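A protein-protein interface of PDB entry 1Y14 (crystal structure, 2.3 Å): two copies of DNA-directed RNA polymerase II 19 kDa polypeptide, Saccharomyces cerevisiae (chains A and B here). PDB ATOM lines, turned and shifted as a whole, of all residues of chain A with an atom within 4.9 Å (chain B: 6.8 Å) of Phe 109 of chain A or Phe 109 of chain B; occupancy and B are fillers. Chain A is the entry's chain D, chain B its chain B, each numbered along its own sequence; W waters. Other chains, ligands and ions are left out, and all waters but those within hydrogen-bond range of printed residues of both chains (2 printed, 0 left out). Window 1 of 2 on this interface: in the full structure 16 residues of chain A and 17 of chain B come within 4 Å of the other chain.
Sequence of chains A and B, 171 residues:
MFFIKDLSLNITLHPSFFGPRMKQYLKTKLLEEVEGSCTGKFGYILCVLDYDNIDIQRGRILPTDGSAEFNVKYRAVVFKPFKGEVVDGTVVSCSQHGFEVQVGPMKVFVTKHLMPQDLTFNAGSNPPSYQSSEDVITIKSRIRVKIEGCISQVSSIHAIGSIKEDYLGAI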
ATOM      1  N   HIS A  97     -20.589 -25.899 -14.260  1.00  0.00           N
ATOM      2  CA  HIS A  97     -20.742 -26.309 -12.865  1.00  0.00           C
ATOM      3  C   HIS A  97     -20.478 -27.805 -12.644  1.00  0.00           C
ATOM      4  O   HIS A  97     -20.227 -28.230 -11.516  1.00  0.00           O
ATOM      5  CB  HIS A  97     -22.148 -25.997 -12.370  1.00  0.00           C
ATOM      6  CG  HIS A  97     -22.519 -24.552 -12.457  1.00  0.00           C
ATOM      7  ND1 HIS A  97     -21.614 -23.533 -12.234  1.00  0.00           N
ATOM      8  CD2 HIS A  97     -23.714 -23.956 -12.680  1.00  0.00           C
ATOM      9  CE1 HIS A  97     -22.239 -22.374 -12.318  1.00  0.00           C
ATOM     10  NE2 HIS A  97     -23.516 -22.603 -12.586  1.00  0.00           N
ATOM     11  N   GLY A  98     -20.542 -28.598 -13.714  1.00  0.00           N
ATOM     12  CA  GLY A  98     -20.298 -30.028 -13.601  1.00  0.00           C
ATOM     13  C   GLY A  98     -21.241 -30.865 -14.457  1.00  0.00           C
ATOM     14  O   GLY A  98     -21.851 -30.359 -15.407  1.00  0.00           O
ATOM     15  N   PHE A  99     -21.387 -32.146 -14.120  1.00  0.00           N
ATOM     16  CA  PHE A  99     -22.266 -33.018 -14.897  1.00  0.00           C
ATOM     17  C   PHE A  99     -23.172 -33.924 -14.067  1.00  0.00           C
ATOM     18  O   PHE A  99     -22.840 -34.295 -12.936  1.00  0.00           O
ATOM     19  CB  PHE A  99     -21.426 -33.860 -15.871  1.00  0.00           C
ATOM     20  CG  PHE A  99     -20.426 -34.773 -15.204  1.00  0.00           C
ATOM     21  CD1 PHE A  99     -20.805 -36.028 -14.735  1.00  0.00           C
ATOM     22  CD2 PHE A  99     -19.088 -34.402 -15.096  1.00  0.00           C
ATOM     23  CE1 PHE A  99     -19.861 -36.904 -14.177  1.00  0.00           C
ATOM     24  CE2 PHE A  99     -18.145 -35.266 -14.541  1.00  0.00           C
ATOM     25  CZ  PHE A  99     -18.534 -36.524 -14.082  1.00  0.00           C
ATOM     26  N   GLU A 100     -24.335 -34.256 -14.627  1.00  0.00           N
ATOM     27  CA  GLU A 100     -25.276 -35.142 -13.951  1.00  0.00           C
ATOM     28  C   GLU A 100     -25.075 -36.566 -14.450  1.00  0.00           C
ATOM     29  O   GLU A 100     -24.760 -36.791 -15.626  1.00  0.00           O
ATOM     30  CB  GLU A 100     -26.737 -34.752 -14.227  1.00  0.00           C
ATOM     31  CG  GLU A 100     -27.219 -33.499 -13.532  1.00  0.00           C
ATOM     32  CD  GLU A 100     -28.716 -33.300 -13.682  1.00  0.00           C
ATOM     33  OE1 GLU A 100     -29.234 -33.508 -14.799  1.00  0.00           O
ATOM     34  OE2 GLU A 100     -29.374 -32.932 -12.684  1.00  0.00           O
ATOM     35  N   LYS A 107     -30.666 -38.630 -10.338  1.00  0.00           N
ATOM     36  CA  LYS A 107     -29.573 -37.954 -11.013  1.00  0.00           C
ATOM     37  C   LYS A 107     -28.573 -37.553  -9.942  1.00  0.00           C
ATOM     38  O   LYS A 107     -28.928 -36.924  -8.945  1.00  0.00           O
ATOM     39  CB  LYS A 107     -30.088 -36.738 -11.788  1.00  0.00           C
ATOM     40  CG  LYS A 107     -30.949 -37.151 -12.989  1.00  0.00           C
ATOM     41  CD  LYS A 107     -31.478 -35.964 -13.772  1.00  0.00           C
ATOM     42  CE  LYS A 107     -32.399 -36.421 -14.884  1.00  0.00           C
ATOM     43  NZ  LYS A 107     -32.949 -35.261 -15.633  1.00  0.00           N
ATOM     44  N   VAL A 108     -27.332 -37.985 -10.120  1.00  0.00           N
ATOM     45  CA  VAL A 108     -26.275 -37.671  -9.174  1.00  0.00           C
ATOM     46  C   VAL A 108     -25.489 -36.542  -9.797  1.00  0.00           C
ATOM     47  O   VAL A 108     -25.019 -36.658 -10.918  1.00  0.00           O
ATOM     48  CB  VAL A 108     -25.330 -38.868  -8.947  1.00  0.00           C
ATOM     49  CG1 VAL A 108     -24.178 -38.458  -8.023  1.00  0.00           C
ATOM     50  CG2 VAL A 108     -26.113 -40.042  -8.345  1.00  0.00           C
ATOM     51  N   PHE A 109     -25.366 -35.437  -9.075  1.00  0.00           N
ATOM     52  CA  PHE A 109     -24.619 -34.316  -9.596  1.00  0.00           C
ATOM     53  C   PHE A 109     -23.189 -34.276  -9.084  1.00  0.00           C
ATOM     54  O   PHE A 109     -22.953 -34.174  -7.876  1.00  0.00           O
ATOM     55  CB  PHE A 109     -25.309 -32.990  -9.261  1.00  0.00           C
ATOM     56  CG  PHE A 109     -24.716 -31.822  -9.988  1.00  0.00           C
ATOM     57  CD1 PHE A 109     -24.718 -31.791 -11.387  1.00  0.00           C
ATOM     58  CD2 PHE A 109     -24.113 -30.776  -9.291  1.00  0.00           C
ATOM     59  CE1 PHE A 109     -24.122 -30.728 -12.092  1.00  0.00           C
ATOM     60  CE2 PHE A 109     -23.512 -29.707  -9.980  1.00  0.00           C
ATOM     61  CZ  PHE A 109     -23.517 -29.684 -11.388  1.00  0.00           C
ATOM     62  N   VAL A 110     -22.242 -34.378 -10.013  1.00  0.00           N
ATOM     63  CA  VAL A 110     -20.823 -34.295  -9.697  1.00  0.00           C
ATOM     64  C   VAL A 110     -20.385 -32.840  -9.950  1.00  0.00           C
ATOM     65  O   VAL A 110     -20.432 -32.369 -11.091  1.00  0.00           O
ATOM     66  CB  VAL A 110     -19.996 -35.217 -10.605  1.00  0.00           C
ATOM     67  CG1 VAL A 110     -18.527 -35.034 -10.307  1.00  0.00           C
ATOM     68  CG2 VAL A 110     -20.409 -36.681 -10.395  1.00  0.00           C
ATOM     69  N   THR A 111     -19.985 -32.118  -8.900  1.00  0.00           N
ATOM     70  CA  THR A 111     -19.555 -30.726  -9.079  1.00  0.00           C
ATOM     71  C   THR A 111     -18.152 -30.681  -9.663  1.00  0.00           C
ATOM     72  O   THR A 111     -17.373 -31.624  -9.501  1.00  0.00           O
ATOM     73  CB  THR A 111     -19.505 -29.944  -7.761  1.00  0.00           C
ATOM     74  OG1 THR A 111     -18.553 -30.559  -6.889  1.00  0.00           O
ATOM     75  CG2 THR A 111     -20.877 -29.901  -7.101  1.00  0.00           C
ATOM     76  N   ALA A 159     -28.559 -36.163  -4.633  1.00  0.00           N
ATOM     77  CA  ALA A 159     -27.246 -36.748  -4.419  1.00  0.00           C
ATOM     78  C   ALA A 159     -26.154 -35.928  -5.085  1.00  0.00           C
ATOM     79  O   ALA A 159     -26.321 -35.443  -6.199  1.00  0.00           O
ATOM     80  CB  ALA A 159     -27.217 -38.169  -4.932  1.00  0.00           C
ATOM     81  N   ILE A 160     -25.044 -35.755  -4.376  1.00  0.00           N
ATOM     82  CA  ILE A 160     -23.908 -35.024  -4.903  1.00  0.00           C
ATOM     83  C   ILE A 160     -22.789 -36.054  -4.970  1.00  0.00           C
ATOM     84  O   ILE A 160     -22.570 -36.784  -4.009  1.00  0.00           O
ATOM     85  CB  ILE A 160     -23.492 -33.879  -3.965  1.00  0.00           C
ATOM     86  CG1 ILE A 160     -24.656 -32.901  -3.783  1.00  0.00           C
ATOM     87  CG2 ILE A 160     -22.290 -33.145  -4.549  1.00  0.00           C
ATOM     88  CD1 ILE A 160     -24.921 -32.025  -4.992  1.00  0.00           C
ATOM     89  N   GLY A 161     -22.080 -36.120  -6.093  1.00  0.00           N
ATOM     90  CA  GLY A 161     -21.026 -37.115  -6.213  1.00  0.00           C
ATOM     91  C   GLY A 161     -19.637 -36.647  -6.589  1.00  0.00           C
ATOM     92  O   GLY A 161     -19.409 -35.486  -6.933  1.00  0.00           O
ATOM     93  N   SER B  93     -22.425 -17.294 -11.061  1.00  0.00           N
ATOM     94  CA  SER B  93     -22.684 -17.914 -12.359  1.00  0.00           C
ATOM     95  C   SER B  93     -23.948 -18.784 -12.367  1.00  0.00           C
ATOM     96  O   SER B  93     -24.339 -19.363 -11.345  1.00  0.00           O
ATOM     97  CB  SER B  93     -21.466 -18.723 -12.815  1.00  0.00           C
ATOM     98  OG  SER B  93     -20.985 -19.566 -11.789  1.00  0.00           O
ATOM     99  N   SER B  95     -26.418 -21.713 -14.742  1.00  0.00           N
ATOM    100  CA  SER B  95     -26.385 -22.775 -15.750  1.00  0.00           C
ATOM    101  C   SER B  95     -27.640 -23.601 -15.610  1.00  0.00           C
ATOM    102  O   SER B  95     -28.450 -23.371 -14.706  1.00  0.00           O
ATOM    103  CB  SER B  95     -25.186 -23.695 -15.569  1.00  0.00           C
ATOM    104  OG  SER B  95     -25.537 -24.779 -14.723  1.00  0.00           O
ATOM    105  N   GLN B  96     -27.791 -24.570 -16.504  1.00  0.00           N
ATOM    106  CA  GLN B  96     -28.951 -25.451 -16.502  1.00  0.00           C
ATOM    107  C   GLN B  96     -28.966 -26.271 -15.209  1.00  0.00           C
ATOM    108  O   GLN B  96     -30.004 -26.784 -14.814  1.00  0.00           O
ATOM    109  CB  GLN B  96     -28.904 -26.388 -17.724  1.00  0.00           C
ATOM    110  CG  GLN B  96     -27.621 -27.202 -17.810  1.00  0.00           C
ATOM    111  CD  GLN B  96     -27.732 -28.426 -18.719  1.00  0.00           C
ATOM    112  OE1 GLN B  96     -28.577 -29.301 -18.514  1.00  0.00           O
ATOM    113  NE2 GLN B  96     -26.867 -28.495 -19.722  1.00  0.00           N
ATOM    114  N   HIS B  97     -27.809 -26.379 -14.558  1.00  0.00           N
ATOM    115  CA  HIS B  97     -27.688 -27.132 -13.310  1.00  0.00           C
ATOM    116  C   HIS B  97     -27.964 -26.344 -12.027  1.00  0.00           C
ATOM    117  O   HIS B  97     -28.132 -26.939 -10.962  1.00  0.00           O
ATOM    118  CB  HIS B  97     -26.302 -27.760 -13.207  1.00  0.00           C
ATOM    119  CG  HIS B  97     -26.007 -28.752 -14.287  1.00  0.00           C
ATOM    120  ND1 HIS B  97     -26.928 -29.685 -14.711  1.00  0.00           N
ATOM    121  CD2 HIS B  97     -24.877 -28.991 -14.992  1.00  0.00           C
ATOM    122  CE1 HIS B  97     -26.377 -30.456 -15.632  1.00  0.00           C
ATOM    123  NE2 HIS B  97     -25.132 -30.057 -15.820  1.00  0.00           N
ATOM    124  N   GLY B  98     -28.015 -25.018 -12.129  1.00  0.00           N
ATOM    125  CA  GLY B  98     -28.275 -24.176 -10.967  1.00  0.00           C
ATOM    126  C   GLY B  98     -27.392 -22.939 -10.972  1.00  0.00           C
ATOM    127  O   GLY B  98     -26.965 -22.500 -12.040  1.00  0.00           O
ATOM    128  N   PHE B  99     -27.114 -22.359  -9.803  1.00  0.00           N
ATOM    129  CA  PHE B  99     -26.249 -21.183  -9.767  1.00  0.00           C
ATOM    130  C   PHE B  99     -25.347 -21.126  -8.543  1.00  0.00           C
ATOM    131  O   PHE B  99     -25.731 -21.573  -7.458  1.00  0.00           O
ATOM    132  CB  PHE B  99     -27.084 -19.897  -9.897  1.00  0.00           C
ATOM    133  CG  PHE B  99     -28.080 -19.685  -8.790  1.00  0.00           C
ATOM    134  CD1 PHE B  99     -27.667 -19.267  -7.522  1.00  0.00           C
ATOM    135  CD2 PHE B  99     -29.439 -19.867  -9.021  1.00  0.00           C
ATOM    136  CE1 PHE B  99     -28.595 -19.034  -6.509  1.00  0.00           C
ATOM    137  CE2 PHE B  99     -30.373 -19.633  -8.013  1.00  0.00           C
ATOM    138  CZ  PHE B  99     -29.952 -19.217  -6.757  1.00  0.00           C
ATOM    139  N   GLU B 100     -24.130 -20.614  -8.741  1.00  0.00           N
ATOM    140  CA  GLU B 100     -23.142 -20.472  -7.664  1.00  0.00           C
ATOM    141  C   GLU B 100     -23.290 -19.137  -6.940  1.00  0.00           C
ATOM    142  O   GLU B 100     -23.436 -18.089  -7.576  1.00  0.00           O
ATOM    143  CB  GLU B 100     -21.708 -20.533  -8.193  1.00  0.00           C
ATOM    144  CG  GLU B 100     -21.140 -21.897  -8.450  1.00  0.00           C
ATOM    145  CD  GLU B 100     -19.659 -21.826  -8.765  1.00  0.00           C
ATOM    146  OE1 GLU B 100     -19.274 -20.989  -9.608  1.00  0.00           O
ATOM    147  OE2 GLU B 100     -18.880 -22.607  -8.179  1.00  0.00           O
ATOM    148  N   VAL B 101     -23.233 -19.191  -5.612  1.00  0.00           N
ATOM    149  CA  VAL B 101     -23.335 -18.002  -4.767  1.00  0.00           C
ATOM    150  C   VAL B 101     -22.021 -17.834  -4.003  1.00  0.00           C
ATOM    151  O   VAL B 101     -21.522 -18.783  -3.396  1.00  0.00           O
ATOM    152  CB  VAL B 101     -24.473 -18.143  -3.734  1.00  0.00           C
ATOM    153  CG1 VAL B 101     -24.542 -16.892  -2.856  1.00  0.00           C
ATOM    154  CG2 VAL B 101     -25.806 -18.365  -4.452  1.00  0.00           C
ATOM    155  N   LYS B 107     -18.011 -20.733  -2.264  1.00  0.00           N
ATOM    156  CA  LYS B 107     -19.097 -20.693  -3.228  1.00  0.00           C
ATOM    157  C   LYS B 107     -20.076 -21.776  -2.809  1.00  0.00           C
ATOM    158  O   LYS B 107     -19.687 -22.902  -2.509  1.00  0.00           O
ATOM    159  CB  LYS B 107     -18.578 -20.945  -4.645  1.00  0.00           C
ATOM    160  CG  LYS B 107     -17.893 -19.723  -5.254  1.00  0.00           C
ATOM    161  CD  LYS B 107     -17.267 -20.027  -6.605  1.00  0.00           C
ATOM    162  CE  LYS B 107     -16.531 -18.810  -7.153  1.00  0.00           C
ATOM    163  NZ  LYS B 107     -15.822 -19.106  -8.432  1.00  0.00           N
ATOM    164  N   VAL B 108     -21.346 -21.409  -2.743  1.00  0.00           N
ATOM    165  CA  VAL B 108     -22.405 -22.330  -2.366  1.00  0.00           C
ATOM    166  C   VAL B 108     -23.181 -22.656  -3.643  1.00  0.00           C
ATOM    167  O   VAL B 108     -23.596 -21.746  -4.358  1.00  0.00           O
ATOM    168  CB  VAL B 108     -23.371 -21.672  -1.350  1.00  0.00           C
ATOM    169  CG1 VAL B 108     -24.572 -22.578  -1.117  1.00  0.00           C
ATOM    170  CG2 VAL B 108     -22.637 -21.390  -0.024  1.00  0.00           C
ATOM    171  N   PHE B 109     -23.368 -23.941  -3.940  1.00  0.00           N
ATOM    172  CA  PHE B 109     -24.111 -24.315  -5.144  1.00  0.00           C
ATOM    173  C   PHE B 109     -25.564 -24.642  -4.856  1.00  0.00           C
ATOM    174  O   PHE B 109     -25.883 -25.535  -4.064  1.00  0.00           O
ATOM    175  CB  PHE B 109     -23.473 -25.507  -5.859  1.00  0.00           C
ATOM    176  CG  PHE B 109     -23.960 -25.678  -7.283  1.00  0.00           C
ATOM    177  CD1 PHE B 109     -23.638 -24.735  -8.254  1.00  0.00           C
ATOM    178  CD2 PHE B 109     -24.768 -26.750  -7.642  1.00  0.00           C
ATOM    179  CE1 PHE B 109     -24.117 -24.856  -9.561  1.00  0.00           C
ATOM    180  CE2 PHE B 109     -25.257 -26.884  -8.955  1.00  0.00           C
ATOM    181  CZ  PHE B 109     -24.928 -25.931  -9.913  1.00  0.00           C
ATOM    182  N   VAL B 110     -26.439 -23.876  -5.486  1.00  0.00           N
ATOM    183  CA  VAL B 110     -27.868 -24.061  -5.360  1.00  0.00           C
ATOM    184  C   VAL B 110     -28.272 -24.826  -6.634  1.00  0.00           C
ATOM    185  O   VAL B 110     -28.314 -24.254  -7.725  1.00  0.00           O
ATOM    186  CB  VAL B 110     -28.580 -22.706  -5.334  1.00  0.00           C
ATOM    187  CG1 VAL B 110     -30.091 -22.908  -5.274  1.00  0.00           C
ATOM    188  CG2 VAL B 110     -28.083 -21.882  -4.162  1.00  0.00           C
ATOM    189  N   THR B 111     -28.531 -26.122  -6.510  1.00  0.00           N
ATOM    190  CA  THR B 111     -28.915 -26.916  -7.679  1.00  0.00           C
ATOM    191  C   THR B 111     -30.308 -26.546  -8.157  1.00  0.00           C
ATOM    192  O   THR B 111     -31.142 -26.078  -7.383  1.00  0.00           O
ATOM    193  CB  THR B 111     -28.954 -28.421  -7.381  1.00  0.00           C
ATOM    194  OG1 THR B 111     -29.985 -28.670  -6.422  1.00  0.00           O
ATOM    195  CG2 THR B 111     -27.632 -28.909  -6.850  1.00  0.00           C
ATOM    196  N   LYS B 112     -30.544 -26.782  -9.445  1.00  0.00           N
ATOM    197  CA  LYS B 112     -31.827 -26.520 -10.090  1.00  0.00           C
ATOM    198  C   LYS B 112     -32.980 -27.175  -9.326  1.00  0.00           C
ATOM    199  O   LYS B 112     -34.098 -26.672  -9.319  1.00  0.00           O
ATOM    200  CB  LYS B 112     -31.792 -27.067 -11.523  1.00  0.00           C
ATOM    201  CG  LYS B 112     -33.118 -27.037 -12.250  1.00  0.00           C
ATOM    202  CD  LYS B 112     -33.078 -27.949 -13.470  1.00  0.00           C
ATOM    203  CE  LYS B 112     -34.452 -28.079 -14.122  1.00  0.00           C
ATOM    204  NZ  LYS B 112     -34.445 -29.022 -15.283  1.00  0.00           N
ATOM    205  N   HIS B 113     -32.705 -28.297  -8.675  1.00  0.00           N
ATOM    206  CA  HIS B 113     -33.752 -29.003  -7.938  1.00  0.00           C
ATOM    207  C   HIS B 113     -34.084 -28.415  -6.571  1.00  0.00           C
ATOM    208  O   HIS B 113     -35.101 -28.763  -5.971  1.00  0.00           O
ATOM    209  CB  HIS B 113     -33.374 -30.480  -7.801  1.00  0.00           C
ATOM    210  CG  HIS B 113     -32.922 -31.100  -9.088  1.00  0.00           C
ATOM    211  ND1 HIS B 113     -31.607 -31.070  -9.507  1.00  0.00           N
ATOM    212  CD2 HIS B 113     -33.618 -31.712 -10.075  1.00  0.00           C
ATOM    213  CE1 HIS B 113     -31.516 -31.636 -10.697  1.00  0.00           C
ATOM    214  NE2 HIS B 113     -32.721 -32.034 -11.065  1.00  0.00           N
ATOM    215  N   LEU B 114     -33.231 -27.520  -6.080  1.00  0.00           N
ATOM    216  CA  LEU B 114     -33.453 -26.886  -4.787  1.00  0.00           C
ATOM    217  C   LEU B 114     -33.914 -25.439  -4.984  1.00  0.00           C
ATOM    218  O   LEU B 114     -33.779 -24.593  -4.094  1.00  0.00           O
ATOM    219  CB  LEU B 114     -32.173 -26.970  -3.943  1.00  0.00           C
ATOM    220  CG  LEU B 114     -31.747 -28.413  -3.593  1.00  0.00           C
ATOM    221  CD1 LEU B 114     -30.375 -28.426  -2.915  1.00  0.00           C
ATOM    222  CD2 LEU B 114     -32.795 -29.040  -2.663  1.00  0.00           C
ATOM    223  N   VAL B 145     -29.710 -17.673   0.884  1.00  0.00           N
ATOM    224  CA  VAL B 145     -29.707 -19.107   0.682  1.00  0.00           C
ATOM    225  C   VAL B 145     -29.575 -19.926   1.978  1.00  0.00           C
ATOM    226  O   VAL B 145     -28.978 -19.479   2.959  1.00  0.00           O
ATOM    227  CB  VAL B 145     -28.542 -19.476  -0.258  1.00  0.00           C
ATOM    228  CG1 VAL B 145     -28.439 -20.974  -0.406  1.00  0.00           C
ATOM    229  CG2 VAL B 145     -28.748 -18.810  -1.611  1.00  0.00           C
ATOM    230  N   HIS B 158     -17.319 -28.058   0.598  1.00  0.00           N
ATOM    231  CA  HIS B 158     -18.280 -27.710  -0.432  1.00  0.00           C
ATOM    232  C   HIS B 158     -19.636 -27.566   0.202  1.00  0.00           C
ATOM    233  O   HIS B 158     -19.962 -28.269   1.153  1.00  0.00           O
ATOM    234  CB  HIS B 158     -18.295 -28.810  -1.491  1.00  0.00           C
ATOM    235  CG  HIS B 158     -16.925 -29.218  -1.922  1.00  0.00           C
ATOM    236  ND1 HIS B 158     -16.312 -28.702  -3.041  1.00  0.00           N
ATOM    237  CD2 HIS B 158     -16.012 -30.021  -1.328  1.00  0.00           C
ATOM    238  CE1 HIS B 158     -15.079 -29.169  -3.120  1.00  0.00           C
ATOM    239  NE2 HIS B 158     -14.871 -29.972  -2.091  1.00  0.00           N
ATOM    240  N   ALA B 159     -20.429 -26.645  -0.316  1.00  0.00           N
ATOM    241  CA  ALA B 159     -21.746 -26.444   0.239  1.00  0.00           C
ATOM    242  C   ALA B 159     -22.823 -26.405  -0.835  1.00  0.00           C
ATOM    243  O   ALA B 159     -22.619 -25.866  -1.929  1.00  0.00           O
ATOM    244  CB  ALA B 159     -21.770 -25.160   1.053  1.00  0.00           C
ATOM    245  N   ILE B 160     -23.963 -27.012  -0.523  1.00  0.00           N
ATOM    246  CA  ILE B 160     -25.097 -27.011  -1.426  1.00  0.00           C
ATOM    247  C   ILE B 160     -26.174 -26.170  -0.747  1.00  0.00           C
ATOM    248  O   ILE B 160     -26.382 -26.278   0.464  1.00  0.00           O
ATOM    249  CB  ILE B 160     -25.628 -28.436  -1.669  1.00  0.00           C
ATOM    250  CG1 ILE B 160     -24.513 -29.331  -2.220  1.00  0.00           C
ATOM    251  CG2 ILE B 160     -26.788 -28.382  -2.627  1.00  0.00           C
ATOM    252  CD1 ILE B 160     -23.906 -28.863  -3.553  1.00  0.00           C
ATOM    253  N   GLY B 161     -26.859 -25.326  -1.512  1.00  0.00           N
ATOM    254  CA  GLY B 161     -27.875 -24.490  -0.900  1.00  0.00           C
ATOM    255  C   GLY B 161     -29.206 -24.565  -1.611  1.00  0.00           C
ATOM    256  O   GLY B 161     -29.307 -25.121  -2.694  1.00  0.00           O
ATOM    257  N   SER B 162     -30.239 -24.007  -1.001  1.00  0.00           N
ATOM    258  CA  SER B 162     -31.543 -24.021  -1.622  1.00  0.00           C
ATOM    259  C   SER B 162     -32.202 -22.696  -1.351  1.00  0.00           C
ATOM    260  O   SER B 162     -31.757 -21.937  -0.474  1.00  0.00           O
ATOM    261  CB  SER B 162     -32.403 -25.159  -1.053  1.00  0.00           C
ATOM    262  OG  SER B 162     -32.663 -24.964   0.314  1.00  0.00           O
HETATM  263  O   HOH W   1     -28.700 -30.285 -10.682  1.00  0.00           O
HETATM  264  O   HOH W   2     -18.396 -28.836  -4.918  1.00  0.00           O
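His 97 of chain A touches Gly 98 of chain B, and with the chains exchanged Gly 98 of chain A touches His 97 of chain B. His 97 of chain A touches Phe 109 of chain B, and with the chains exchanged Phe 109 of chain A touches His 97 of chain B. Glu 100 of chain A touches His 97 of chain B, but with the chains exchanged His 97 of chain A does not touch Glu 100 of chain B (4.05 Å). Phe 109 of chain B touches its own counterpart, Phe 109 of chain A. Positions printed for both chains: 97, 98, 99, 100, 107, 108, 109, 110, 111, 159, 160 and 161. Of the 10 pairs that touch across the chains among the printed residues, 6 have their exchanged pair printed and touching as well.
Of the 22 printed residues of chain B, 7 touch a printed residue of chain A. Hydrophobic or aromatic side chains of chain B that line the printed part of chain A: His 97, Phe 109, His 113 and Ile 160. Hydrophobic or aromatic side chains of chain A within 4 Å of the printed part of chain B: His 97, Phe 109 and Ile 160.
O of Gly 98 of chain B sits at hydrogen-bond distance from NE2 of His 97 of chain A. A ring nitrogen (NE2) of His 97 of chain B lies within hydrogen-bond range of the backbone carbonyl oxygen of Gly 98 of chain A (3.3 Å).
N of Phe 109 of chain B sits at hydrogen-bond distance from O of Ala 159 of chain B (2.9 Å). OG of Ser 95 of chain B sits at hydrogen-bond distance from N of His 97 of chain B (2.8 Å). N of Phe 109 of chain A lies within hydrogen-bond range of O of Ala 159 of chain A (3.0 Å). The backbone carbonyl oxygen (O) of Ser 93 of chain B sits at hydrogen-bond distance from the backbone NH (N) of Glu 100 of chain B (2.9 Å). The backbone carbonyl oxygen (O) of His 97 of chain B is in hydrogen-bond range of the backbone NH (N) of Lys 112 of chain B (2.9 Å). The backbone carbonyl oxygen (O) of Phe 109 of chain B sits at hydrogen-bond distance from the backbone NH (N) of Gly 161 of chain B, at 2.7 Å.
Water W2 lies within hydrogen-bond range of OG1 of Thr 111 of chain A (2.6 Å) and ND1 of His 158 of chain B (2.8 Å). Water W1 lies within hydrogen-bond range of a ring nitrogen (ND1) of His 113 of chain B (3.2 Å), the side-chain carboxylate of Glu 100 of chain A (3.4 Å) and the backbone carbonyl oxygen of His 97 of chain B (3.4 Å).
Of chain B, only His 97 and Phe 109 come within 4 Å of Phe 109 of chain A. Phe 109 of chain B touches two residues of chain A. Of the printed residues of chain A, His 97 of chain B touches Gly 98 (3.3 Å), Glu 100 (3.8 Å) and Phe 109 (3.5 Å). Of the printed residues of chain B, Gly 98 of chain A touches His 97 (3.3 Å). Printed residues of chain A within 4 Å of Ile 160 of chain B: Ile 160 (3.6 Å). Printed residues of chain A within 4 Å of Ser 95 of chain B: His 97 (2.9 Å). Printed residues of chain B within 4 Å of His 97 of chain A: Ser 93, Ser 95, Gly 98 and Phe 109. Gly 161 of chain B touches none of the printed residues of chain A. The nearest printed residue of chain B that does not touch His 97 of chain A is Glu 100 of chain B (4.05 Å).
Ser 93 of chain B touches His 97 of chain A. Ser 95 of chain B touches His 97 of chain A (OG to CD2, 2.9 Å). Phe 109 of chain B touches His 97 of chain A (CE1 to CD2, 3.3 Å). CG of Glu 100 of chain A touches CE1 of His 97 of chain B (3.8 Å). Glu 100 of chain A touches His 113 of chain B (OE2 to CE1, 3.2 Å). His 97 of chain B touches Phe 109 of chain A. Phe 109 of chain A touches Phe 109 of chain B (CE2 to CE2, 3.5 Å). Ile 160 of chain B touches Ile 160 of chain A (CD1 to CD1, 3.6 Å).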
